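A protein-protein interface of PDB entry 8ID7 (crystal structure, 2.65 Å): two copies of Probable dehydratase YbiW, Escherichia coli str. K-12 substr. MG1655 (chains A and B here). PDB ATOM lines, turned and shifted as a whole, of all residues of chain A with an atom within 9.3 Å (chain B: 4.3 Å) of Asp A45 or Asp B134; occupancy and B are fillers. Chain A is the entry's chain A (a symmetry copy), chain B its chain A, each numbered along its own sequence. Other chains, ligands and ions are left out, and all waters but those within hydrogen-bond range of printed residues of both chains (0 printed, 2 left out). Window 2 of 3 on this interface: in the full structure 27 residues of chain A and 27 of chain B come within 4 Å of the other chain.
Of chain A, only Asp A45 (3.4 Å) comes within 4 Å of Asp B134.
Of the printed residues of chain A, Gly B129 touches Leu A44 (3.4 Å) and Asp A45 (3.3 Å).
Printed residues of chain A within 4 Å of Gly B138: Asp A45, Lys A46 and Pro A47.
Of the printed residues of chain B, Arg A51 touches Arg B135 (3.7 Å).
Of the printed residues of chain B, Pro A47 touches Gly B138.
Printed residues of chain B within 4 Å of Leu A44: Gly B129 (3.4 Å) and Arg B135 (2.9 Å).
The nearest printed residue of chain B that does not touch Asp A45 is Tyr B137 (4.4 Å).
The nearest printed residue of chain B that does not touch Arg A51 is Gly B129 (6.5 Å).
The backbone carbonyl oxygen (O) of Gly B129 lies close to the backbone NH (N) of Asp A45 (3.4 Å).
NH2 of Arg B135 lies within hydrogen-bond range of O of Leu A44, 2.9 Å away.
O of Gly B129 sits close to O of Leu A44 (3.4 Å).
No position is printed for both chains.
Of the 9 pairs that touch across the chains among the printed residues, none has its exchanged pair printed and touching as well.
Among the printed residues, merely in contact across the chains: Asp A45 with Gly B138 (3.3 Å), Asp A45 with Asp B134 (3.4 Å), Lys A46 with Gly B138 (3.6 Å), Arg A51 with Arg B135 (3.7 Å), Asp A45 with Arg B135 (3.9 Å) and Pro A47 with Gly B138 (3.9 Å).
Of the 18 printed residues of chain A, 5 touch a printed residue of chain B.
Hydrophobic or aromatic side chains of chain A that line the printed part of chain B: Leu A44 and Pro A47.
Along chain A the printed residues that touch a printed residue of chain B span positions 44 to 51.
Among the printed residues, no Asp or Glu carboxylate lies within 4 Å of a Lys or Arg side-chain nitrogen of the other chain.
The backbone NH (N) of Gly B129 sits at hydrogen-bond distance from the side-chain carboxylate (OD2) of Asp B134 (2.4 Å).
The side-chain hydroxyl (OG1) of Thr B131 sits close to the side-chain carboxylate (OD1) of Asp B134, at 3.4 Å.
The side-chain amino group of Lys A46 lies close to a ring nitrogen (ND1) of His A43 (3.5 Å).
The backbone carbonyl oxygen of His A43 lies within hydrogen-bond range of the guanidinium group of Arg A51, at 3.3 Å.
The guanidinium group (NH2) of Arg A51 is in hydrogen-bond range of the backbone carbonyl oxygen (O) of Leu A44, at 3.4 Å.
The backbone carbonyl oxygen (O) of Lys A46 is in hydrogen-bond range of the guanidinium group (NH2) of Arg A51, 3.1 Å away.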
ATOM      1  N   GLU A  38       2.204  27.254   6.683  1.00  0.00           N
ATOM      2  CA  GLU A  38       1.720  26.461   7.803  1.00  0.00           C
ATOM      3  C   GLU A  38       2.854  25.699   8.474  1.00  0.00           C
ATOM      4  O   GLU A  38       3.121  25.875   9.663  1.00  0.00           O
ATOM      5  CB  GLU A  38       0.657  25.481   7.316  1.00  0.00           C
ATOM      6  CG  GLU A  38      -0.439  26.085   6.488  1.00  0.00           C
ATOM      7  CD  GLU A  38      -1.397  25.023   6.003  1.00  0.00           C
ATOM      8  OE1 GLU A  38      -1.317  23.896   6.545  1.00  0.00           O
ATOM      9  OE2 GLU A  38      -2.207  25.300   5.080  1.00  0.00           O
ATOM     10  N   MET A  39       3.512  24.822   7.714  1.00  0.00           N
ATOM     11  CA  MET A  39       4.555  23.967   8.265  1.00  0.00           C
ATOM     12  C   MET A  39       5.711  24.778   8.827  1.00  0.00           C
ATOM     13  O   MET A  39       6.297  24.398   9.848  1.00  0.00           O
ATOM     14  CB  MET A  39       5.045  23.000   7.193  1.00  0.00           C
ATOM     15  CG  MET A  39       3.989  22.002   6.772  1.00  0.00           C
ATOM     16  SD  MET A  39       3.312  21.107   8.202  1.00  0.00           S
ATOM     17  CE  MET A  39       2.152  22.319   8.839  1.00  0.00           C
ATOM     18  N   TYR A  40       6.071  25.895   8.175  1.00  0.00           N
ATOM     19  CA  TYR A  40       7.047  26.800   8.778  1.00  0.00           C
ATOM     20  C   TYR A  40       6.509  27.449  10.041  1.00  0.00           C
ATOM     21  O   TYR A  40       7.293  27.951  10.855  1.00  0.00           O
ATOM     22  CB  TYR A  40       7.468  27.896   7.801  1.00  0.00           C
ATOM     23  CG  TYR A  40       8.679  27.560   6.958  1.00  0.00           C
ATOM     24  CD1 TYR A  40       8.629  26.555   5.999  1.00  0.00           C
ATOM     25  CD2 TYR A  40       9.862  28.267   7.106  1.00  0.00           C
ATOM     26  CE1 TYR A  40       9.730  26.258   5.220  1.00  0.00           C
ATOM     27  CE2 TYR A  40      10.960  27.981   6.345  1.00  0.00           C
ATOM     28  CZ  TYR A  40      10.900  26.975   5.403  1.00  0.00           C
ATOM     29  OH  TYR A  40      12.006  26.691   4.627  1.00  0.00           O
ATOM     30  N   GLN A  41       5.194  27.457  10.221  1.00  0.00           N
ATOM     31  CA  GLN A  41       4.589  28.046  11.401  1.00  0.00           C
ATOM     32  C   GLN A  41       4.314  27.023  12.489  1.00  0.00           C
ATOM     33  O   GLN A  41       4.270  27.389  13.673  1.00  0.00           O
ATOM     34  CB  GLN A  41       3.296  28.769  11.004  1.00  0.00           C
ATOM     35  CG  GLN A  41       3.567  30.189  10.522  1.00  0.00           C
ATOM     36  CD  GLN A  41       2.530  30.704   9.577  1.00  0.00           C
ATOM     37  OE1 GLN A  41       1.607  29.984   9.197  1.00  0.00           O
ATOM     38  NE2 GLN A  41       2.668  31.958   9.187  1.00  0.00           N
ATOM     39  N   GLN A  42       4.161  25.756  12.104  1.00  0.00           N
ATOM     40  CA  GLN A  42       3.918  24.635  13.002  1.00  0.00           C
ATOM     41  C   GLN A  42       5.206  23.999  13.474  1.00  0.00           C
ATOM     42  O   GLN A  42       5.251  23.469  14.588  1.00  0.00           O
ATOM     43  CB  GLN A  42       3.052  23.580  12.295  1.00  0.00           C
ATOM     44  CG  GLN A  42       3.020  22.176  12.929  1.00  0.00           C
ATOM     45  CD  GLN A  42       1.831  21.323  12.411  1.00  0.00           C
ATOM     46  OE1 GLN A  42       0.877  21.858  11.828  1.00  0.00           O
ATOM     47  NE2 GLN A  42       1.899  19.999  12.616  1.00  0.00           N
ATOM     48  N   HIS A  43       6.261  24.070  12.670  1.00  0.00           N
ATOM     49  CA  HIS A  43       7.525  23.420  12.970  1.00  0.00           C
ATOM     50  C   HIS A  43       8.673  24.415  13.020  1.00  0.00           C
ATOM     51  O   HIS A  43       9.802  24.100  12.641  1.00  0.00           O
ATOM     52  CB  HIS A  43       7.803  22.321  11.955  1.00  0.00           C
ATOM     53  CG  HIS A  43       6.784  21.232  11.971  1.00  0.00           C
ATOM     54  ND1 HIS A  43       6.845  20.170  12.847  1.00  0.00           N
ATOM     55  CD2 HIS A  43       5.662  21.048  11.236  1.00  0.00           C
ATOM     56  CE1 HIS A  43       5.815  19.371  12.639  1.00  0.00           C
ATOM     57  NE2 HIS A  43       5.082  19.880  11.666  1.00  0.00           N
ATOM     58  N   LEU A  44       8.395  25.631  13.501  1.00  0.00           N
ATOM     59  CA  LEU A  44       9.448  26.630  13.656  1.00  0.00           C
ATOM     60  C   LEU A  44      10.606  26.111  14.484  1.00  0.00           C
ATOM     61  O   LEU A  44      11.740  26.580  14.322  1.00  0.00           O
ATOM     62  CB  LEU A  44       8.894  27.890  14.310  1.00  0.00           C
ATOM     63  CG  LEU A  44       8.801  29.134  13.429  1.00  0.00           C
ATOM     64  CD1 LEU A  44       8.754  30.399  14.278  1.00  0.00           C
ATOM     65  CD2 LEU A  44       9.986  29.170  12.504  1.00  0.00           C
ATOM     66  N   ASP A  45      10.333  25.166  15.394  1.00  0.00           N
ATOM     67  CA  ASP A  45      11.324  24.597  16.299  1.00  0.00           C
ATOM     68  C   ASP A  45      12.219  23.562  15.632  1.00  0.00           C
ATOM     69  O   ASP A  45      13.200  23.129  16.249  1.00  0.00           O
ATOM     70  CB  ASP A  45      10.627  23.960  17.506  1.00  0.00           C
ATOM     71  CG  ASP A  45       9.612  22.899  17.103  1.00  0.00           C
ATOM     72  OD1 ASP A  45       8.871  23.122  16.120  1.00  0.00           O
ATOM     73  OD2 ASP A  45       9.556  21.829  17.751  1.00  0.00           O
ATOM     74  N   LYS A  46      11.896  23.132  14.356  1.00  0.00           N
ATOM     75  CA  LYS A  46      12.778  22.103  13.825  1.00  0.00           C
ATOM     76  C   LYS A  46      13.984  22.715  13.125  1.00  0.00           C
ATOM     77  O   LYS A  46      13.925  23.850  12.637  1.00  0.00           O
ATOM     78  CB  LYS A  46      12.032  21.194  12.839  1.00  0.00           C
ATOM     79  CG  LYS A  46      10.644  20.737  13.296  1.00  0.00           C
ATOM     80  CD  LYS A  46      10.662  19.753  14.461  1.00  0.00           C
ATOM     81  CE  LYS A  46       9.227  19.451  14.944  1.00  0.00           C
ATOM     82  NZ  LYS A  46       8.599  20.493  15.846  1.00  0.00           N
ATOM     83  N   PRO A  47      15.078  21.962  13.071  1.00  0.00           N
ATOM     84  CA  PRO A  47      16.129  22.272  12.094  1.00  0.00           C
ATOM     85  C   PRO A  47      15.510  22.471  10.719  1.00  0.00           C
ATOM     86  O   PRO A  47      14.554  21.797  10.338  1.00  0.00           O
ATOM     87  CB  PRO A  47      17.039  21.038  12.115  1.00  0.00           C
ATOM     88  CG  PRO A  47      16.571  20.198  13.231  1.00  0.00           C
ATOM     89  CD  PRO A  47      15.191  20.600  13.612  1.00  0.00           C
ATOM     90  N   ILE A  48      16.086  23.396   9.962  1.00  0.00           N
ATOM     91  CA  ILE A  48      15.504  23.713   8.661  1.00  0.00           C
ATOM     92  C   ILE A  48      15.404  22.496   7.773  1.00  0.00           C
ATOM     93  O   ILE A  48      14.352  22.301   7.148  1.00  0.00           O
ATOM     94  CB  ILE A  48      16.279  24.898   8.031  1.00  0.00           C
ATOM     95  CG1 ILE A  48      15.983  26.163   8.862  1.00  0.00           C
ATOM     96  CG2 ILE A  48      15.858  25.064   6.585  1.00  0.00           C
ATOM     97  CD1 ILE A  48      17.169  27.166   9.046  1.00  0.00           C
ATOM     98  N   PRO A  49      16.384  21.593   7.693  1.00  0.00           N
ATOM     99  CA  PRO A  49      16.190  20.424   6.819  1.00  0.00           C
ATOM    100  C   PRO A  49      14.960  19.618   7.174  1.00  0.00           C
ATOM    101  O   PRO A  49      14.322  19.074   6.265  1.00  0.00           O
ATOM    102  CB  PRO A  49      17.476  19.603   6.996  1.00  0.00           C
ATOM    103  CG  PRO A  49      18.192  20.225   8.136  1.00  0.00           C
ATOM    104  CD  PRO A  49      17.741  21.637   8.266  1.00  0.00           C
ATOM    105  N   VAL A  50      14.588  19.526   8.456  1.00  0.00           N
ATOM    106  CA  VAL A  50      13.426  18.714   8.798  1.00  0.00           C
ATOM    107  C   VAL A  50      12.161  19.507   8.589  1.00  0.00           C
ATOM    108  O   VAL A  50      11.184  18.992   8.034  1.00  0.00           O
ATOM    109  CB  VAL A  50      13.517  18.181  10.235  1.00  0.00           C
ATOM    110  CG1 VAL A  50      12.131  17.850  10.750  1.00  0.00           C
ATOM    111  CG2 VAL A  50      14.409  16.954  10.288  1.00  0.00           C
ATOM    112  N   ARG A  51      12.158  20.770   9.021  1.00  0.00           N
ATOM    113  CA  ARG A  51      11.008  21.635   8.784  1.00  0.00           C
ATOM    114  C   ARG A  51      10.621  21.636   7.302  1.00  0.00           C
ATOM    115  O   ARG A  51       9.447  21.510   6.949  1.00  0.00           O
ATOM    116  CB  ARG A  51      11.320  23.047   9.270  1.00  0.00           C
ATOM    117  CG  ARG A  51      10.161  24.018   9.126  1.00  0.00           C
ATOM    118  CD  ARG A  51      10.546  25.466   9.565  1.00  0.00           C
ATOM    119  NE  ARG A  51      11.727  25.565  10.430  1.00  0.00           N
ATOM    120  CZ  ARG A  51      12.423  26.683  10.626  1.00  0.00           C
ATOM    121  NH1 ARG A  51      12.063  27.795  10.023  1.00  0.00           N
ATOM    122  NH2 ARG A  51      13.485  26.696  11.423  1.00  0.00           N
ATOM    123  N   LEU A  54       9.004  18.442   6.184  1.00  0.00           N
ATOM    124  CA  LEU A  54       7.607  18.337   6.585  1.00  0.00           C
ATOM    125  C   LEU A  54       6.719  19.142   5.647  1.00  0.00           C
ATOM    126  O   LEU A  54       5.771  18.606   5.055  1.00  0.00           O
ATOM    127  CB  LEU A  54       7.440  18.804   8.029  1.00  0.00           C
ATOM    128  CG  LEU A  54       8.179  17.970   9.086  1.00  0.00           C
ATOM    129  CD1 LEU A  54       7.977  18.566  10.457  1.00  0.00           C
ATOM    130  CD2 LEU A  54       7.773  16.494   9.066  1.00  0.00           C
ATOM    131  N   TRP A 126       4.745  37.602   6.450  1.00  0.00           N
ATOM    132  CA  TRP A 126       5.402  36.791   7.463  1.00  0.00           C
ATOM    133  C   TRP A 126       6.775  36.353   7.013  1.00  0.00           C
ATOM    134  O   TRP A 126       7.702  36.289   7.822  1.00  0.00           O
ATOM    135  CB  TRP A 126       4.560  35.557   7.792  1.00  0.00           C
ATOM    136  CG  TRP A 126       5.119  34.751   8.925  1.00  0.00           C
ATOM    137  CD1 TRP A 126       5.010  35.021  10.265  1.00  0.00           C
ATOM    138  CD2 TRP A 126       5.884  33.550   8.816  1.00  0.00           C
ATOM    139  NE1 TRP A 126       5.667  34.054  10.996  1.00  0.00           N
ATOM    140  CE2 TRP A 126       6.207  33.138  10.124  1.00  0.00           C
ATOM    141  CE3 TRP A 126       6.329  32.782   7.741  1.00  0.00           C
ATOM    142  CZ2 TRP A 126       6.956  31.986  10.377  1.00  0.00           C
ATOM    143  CZ3 TRP A 126       7.070  31.641   7.995  1.00  0.00           C
ATOM    144  CH2 TRP A 126       7.377  31.254   9.296  1.00  0.00           C
ATOM    145  N   GLN A 204      20.013  15.093  11.531  1.00  0.00           N
ATOM    146  CA  GLN A 204      18.869  15.919  11.154  1.00  0.00           C
ATOM    147  C   GLN A 204      18.655  15.838   9.651  1.00  0.00           C
ATOM    148  O   GLN A 204      17.548  15.580   9.177  1.00  0.00           O
ATOM    149  CB  GLN A 204      19.043  17.379  11.596  1.00  0.00           C
ATOM    150  CG  GLN A 204      18.903  17.659  13.096  1.00  0.00           C
ATOM    151  CD  GLN A 204      17.833  16.817  13.783  1.00  0.00           C
ATOM    152  OE1 GLN A 204      17.983  15.603  13.906  1.00  0.00           O
ATOM    153  NE2 GLN A 204      16.760  17.459  14.242  1.00  0.00           N
ATOM    154  N   LYS A 207      17.275  12.384   9.014  1.00  0.00           N
ATOM    155  CA  LYS A 207      15.873  12.398   9.408  1.00  0.00           C
ATOM    156  C   LYS A 207      15.024  13.000   8.304  1.00  0.00           C
ATOM    157  O   LYS A 207      14.005  12.429   7.895  1.00  0.00           O
ATOM    158  CB  LYS A 207      15.699  13.192  10.702  1.00  0.00           C
ATOM    159  CG  LYS A 207      14.752  12.565  11.701  1.00  0.00           C
ATOM    160  CD  LYS A 207      14.597  13.436  12.943  1.00  0.00           C
ATOM    161  CE  LYS A 207      13.329  14.282  12.835  1.00  0.00           C
ATOM    162  NZ  LYS A 207      12.601  14.499  14.143  1.00  0.00           N
ATOM    163  N   SER B  93       8.477  29.480  27.849  1.00  0.00           N
ATOM    164  CA  SER B  93       7.489  28.484  28.247  1.00  0.00           C
ATOM    165  C   SER B  93       7.113  28.587  29.719  1.00  0.00           C
ATOM    166  O   SER B  93       5.931  28.521  30.056  1.00  0.00           O
ATOM    167  CB  SER B  93       7.989  27.083  27.921  1.00  0.00           C
ATOM    168  OG  SER B  93       7.506  26.704  26.643  1.00  0.00           O
ATOM    169  N   ARG B 128       7.698  32.160  20.733  1.00  0.00           N
ATOM    170  CA  ARG B 128       7.333  30.751  20.705  1.00  0.00           C
ATOM    171  C   ARG B 128       7.881  30.105  19.441  1.00  0.00           C
ATOM    172  O   ARG B 128       7.803  30.682  18.353  1.00  0.00           O
ATOM    173  CB  ARG B 128       5.811  30.575  20.766  1.00  0.00           C
ATOM    174  CG  ARG B 128       5.118  31.172  22.003  1.00  0.00           C
ATOM    175  CD  ARG B 128       3.630  30.779  22.050  1.00  0.00           C
ATOM    176  NE  ARG B 128       2.845  31.619  22.955  1.00  0.00           N
ATOM    177  CZ  ARG B 128       1.556  31.906  22.781  1.00  0.00           C
ATOM    178  NH1 ARG B 128       0.903  31.421  21.729  1.00  0.00           N
ATOM    179  NH2 ARG B 128       0.920  32.681  23.649  1.00  0.00           N
ATOM    180  N   GLY B 129       8.464  28.914  19.591  1.00  0.00           N
ATOM    181  CA  GLY B 129       9.026  28.186  18.478  1.00  0.00           C
ATOM    182  C   GLY B 129      10.459  28.535  18.110  1.00  0.00           C
ATOM    183  O   GLY B 129      11.114  27.732  17.435  1.00  0.00           O
ATOM    184  N   THR B 131      12.913  29.865  20.498  1.00  0.00           N
ATOM    185  CA  THR B 131      13.800  29.964  21.650  1.00  0.00           C
ATOM    186  C   THR B 131      14.659  28.706  21.801  1.00  0.00           C
ATOM    187  O   THR B 131      14.290  27.612  21.352  1.00  0.00           O
ATOM    188  CB  THR B 131      13.005  30.195  22.933  1.00  0.00           C
ATOM    189  OG1 THR B 131      11.790  29.444  22.870  1.00  0.00           O
ATOM    190  CG2 THR B 131      12.692  31.679  23.108  1.00  0.00           C
ATOM    191  N   VAL B 132      15.826  28.890  22.431  1.00  0.00           N
ATOM    192  CA  VAL B 132      16.760  27.818  22.772  1.00  0.00           C
ATOM    193  C   VAL B 132      15.997  26.607  23.298  1.00  0.00           C
ATOM    194  O   VAL B 132      16.120  25.502  22.761  1.00  0.00           O
ATOM    195  CB  VAL B 132      17.795  28.318  23.802  1.00  0.00           C
ATOM    196  CG1 VAL B 132      18.932  27.325  24.011  1.00  0.00           C
ATOM    197  CG2 VAL B 132      18.356  29.642  23.359  1.00  0.00           C
ATOM    198  N   GLN B 133      15.198  26.809  24.347  1.00  0.00           N
ATOM    199  CA  GLN B 133      14.434  25.705  24.919  1.00  0.00           C
ATOM    200  C   GLN B 133      13.485  25.093  23.880  1.00  0.00           C
ATOM    201  O   GLN B 133      13.484  23.871  23.664  1.00  0.00           O
ATOM    202  CB  GLN B 133      13.698  26.199  26.182  1.00  0.00           C
ATOM    203  CG  GLN B 133      12.830  25.190  26.931  1.00  0.00           C
ATOM    204  CD  GLN B 133      12.550  25.601  28.383  1.00  0.00           C
ATOM    205  OE1 GLN B 133      12.061  26.707  28.677  1.00  0.00           O
ATOM    206  NE2 GLN B 133      12.856  24.695  29.300  1.00  0.00           N
ATOM    207  N   ASP B 134      12.690  25.933  23.203  1.00  0.00           N
ATOM    208  CA  ASP B 134      11.748  25.423  22.208  1.00  0.00           C
ATOM    209  C   ASP B 134      12.464  24.575  21.167  1.00  0.00           C
ATOM    210  O   ASP B 134      11.917  23.574  20.676  1.00  0.00           O
ATOM    211  CB  ASP B 134      11.030  26.579  21.518  1.00  0.00           C
ATOM    212  CG  ASP B 134       9.728  26.960  22.191  1.00  0.00           C
ATOM    213  OD1 ASP B 134       9.641  26.832  23.430  1.00  0.00           O
ATOM    214  OD2 ASP B 134       8.792  27.402  21.478  1.00  0.00           O
ATOM    215  N   ARG B 135      13.691  24.972  20.809  1.00  0.00           N
ATOM    216  CA  ARG B 135      14.398  24.313  19.722  1.00  0.00           C
ATOM    217  C   ARG B 135      15.083  23.043  20.204  1.00  0.00           C
ATOM    218  O   ARG B 135      15.044  22.016  19.521  1.00  0.00           O
ATOM    219  CB  ARG B 135      15.389  25.288  19.088  1.00  0.00           C
ATOM    220  CG  ARG B 135      14.714  26.354  18.213  1.00  0.00           C
ATOM    221  CD  ARG B 135      15.347  26.455  16.820  1.00  0.00           C
ATOM    222  NE  ARG B 135      14.459  27.050  15.815  1.00  0.00           N
ATOM    223  CZ  ARG B 135      14.514  28.314  15.395  1.00  0.00           C
ATOM    224  NH1 ARG B 135      15.416  29.166  15.881  1.00  0.00           N
ATOM    225  NH2 ARG B 135      13.658  28.728  14.471  1.00  0.00           N
ATOM    226  N   CYS B 136      15.699  23.078  21.379  1.00  0.00           N
ATOM    227  CA  CYS B 136      16.147  21.829  21.969  1.00  0.00           C
ATOM    228  C   CYS B 136      15.064  20.756  21.820  1.00  0.00           C
ATOM    229  O   CYS B 136      15.328  19.651  21.325  1.00  0.00           O
ATOM    230  CB  CYS B 136      16.539  22.062  23.429  1.00  0.00           C
ATOM    231  SG  CYS B 136      18.036  23.062  23.597  1.00  0.00           S
ATOM    232  N   TYR B 137      13.819  21.086  22.185  1.00  0.00           N
ATOM    233  CA  TYR B 137      12.728  20.127  22.008  1.00  0.00           C
ATOM    234  C   TYR B 137      12.384  19.872  20.541  1.00  0.00           C
ATOM    235  O   TYR B 137      11.790  18.832  20.223  1.00  0.00           O
ATOM    236  CB  TYR B 137      11.493  20.589  22.779  1.00  0.00           C
ATOM    237  CG  TYR B 137      11.679  20.341  24.250  1.00  0.00           C
ATOM    238  CD1 TYR B 137      12.286  21.279  25.060  1.00  0.00           C
ATOM    239  CD2 TYR B 137      11.308  19.134  24.816  1.00  0.00           C
ATOM    240  CE1 TYR B 137      12.481  21.033  26.404  1.00  0.00           C
ATOM    241  CE2 TYR B 137      11.491  18.885  26.148  1.00  0.00           C
ATOM    242  CZ  TYR B 137      12.081  19.827  26.940  1.00  0.00           C
ATOM    243  OH  TYR B 137      12.267  19.551  28.286  1.00  0.00           O
ATOM    244  N   GLY B 138      12.762  20.781  19.641  1.00  0.00           N
ATOM    245  CA  GLY B 138      12.653  20.485  18.221  1.00  0.00           C
ATOM    246  C   GLY B 138      13.625  19.429  17.728  1.00  0.00           C
ATOM    247  O   GLY B 138      13.417  18.868  16.646  1.00  0.00           O
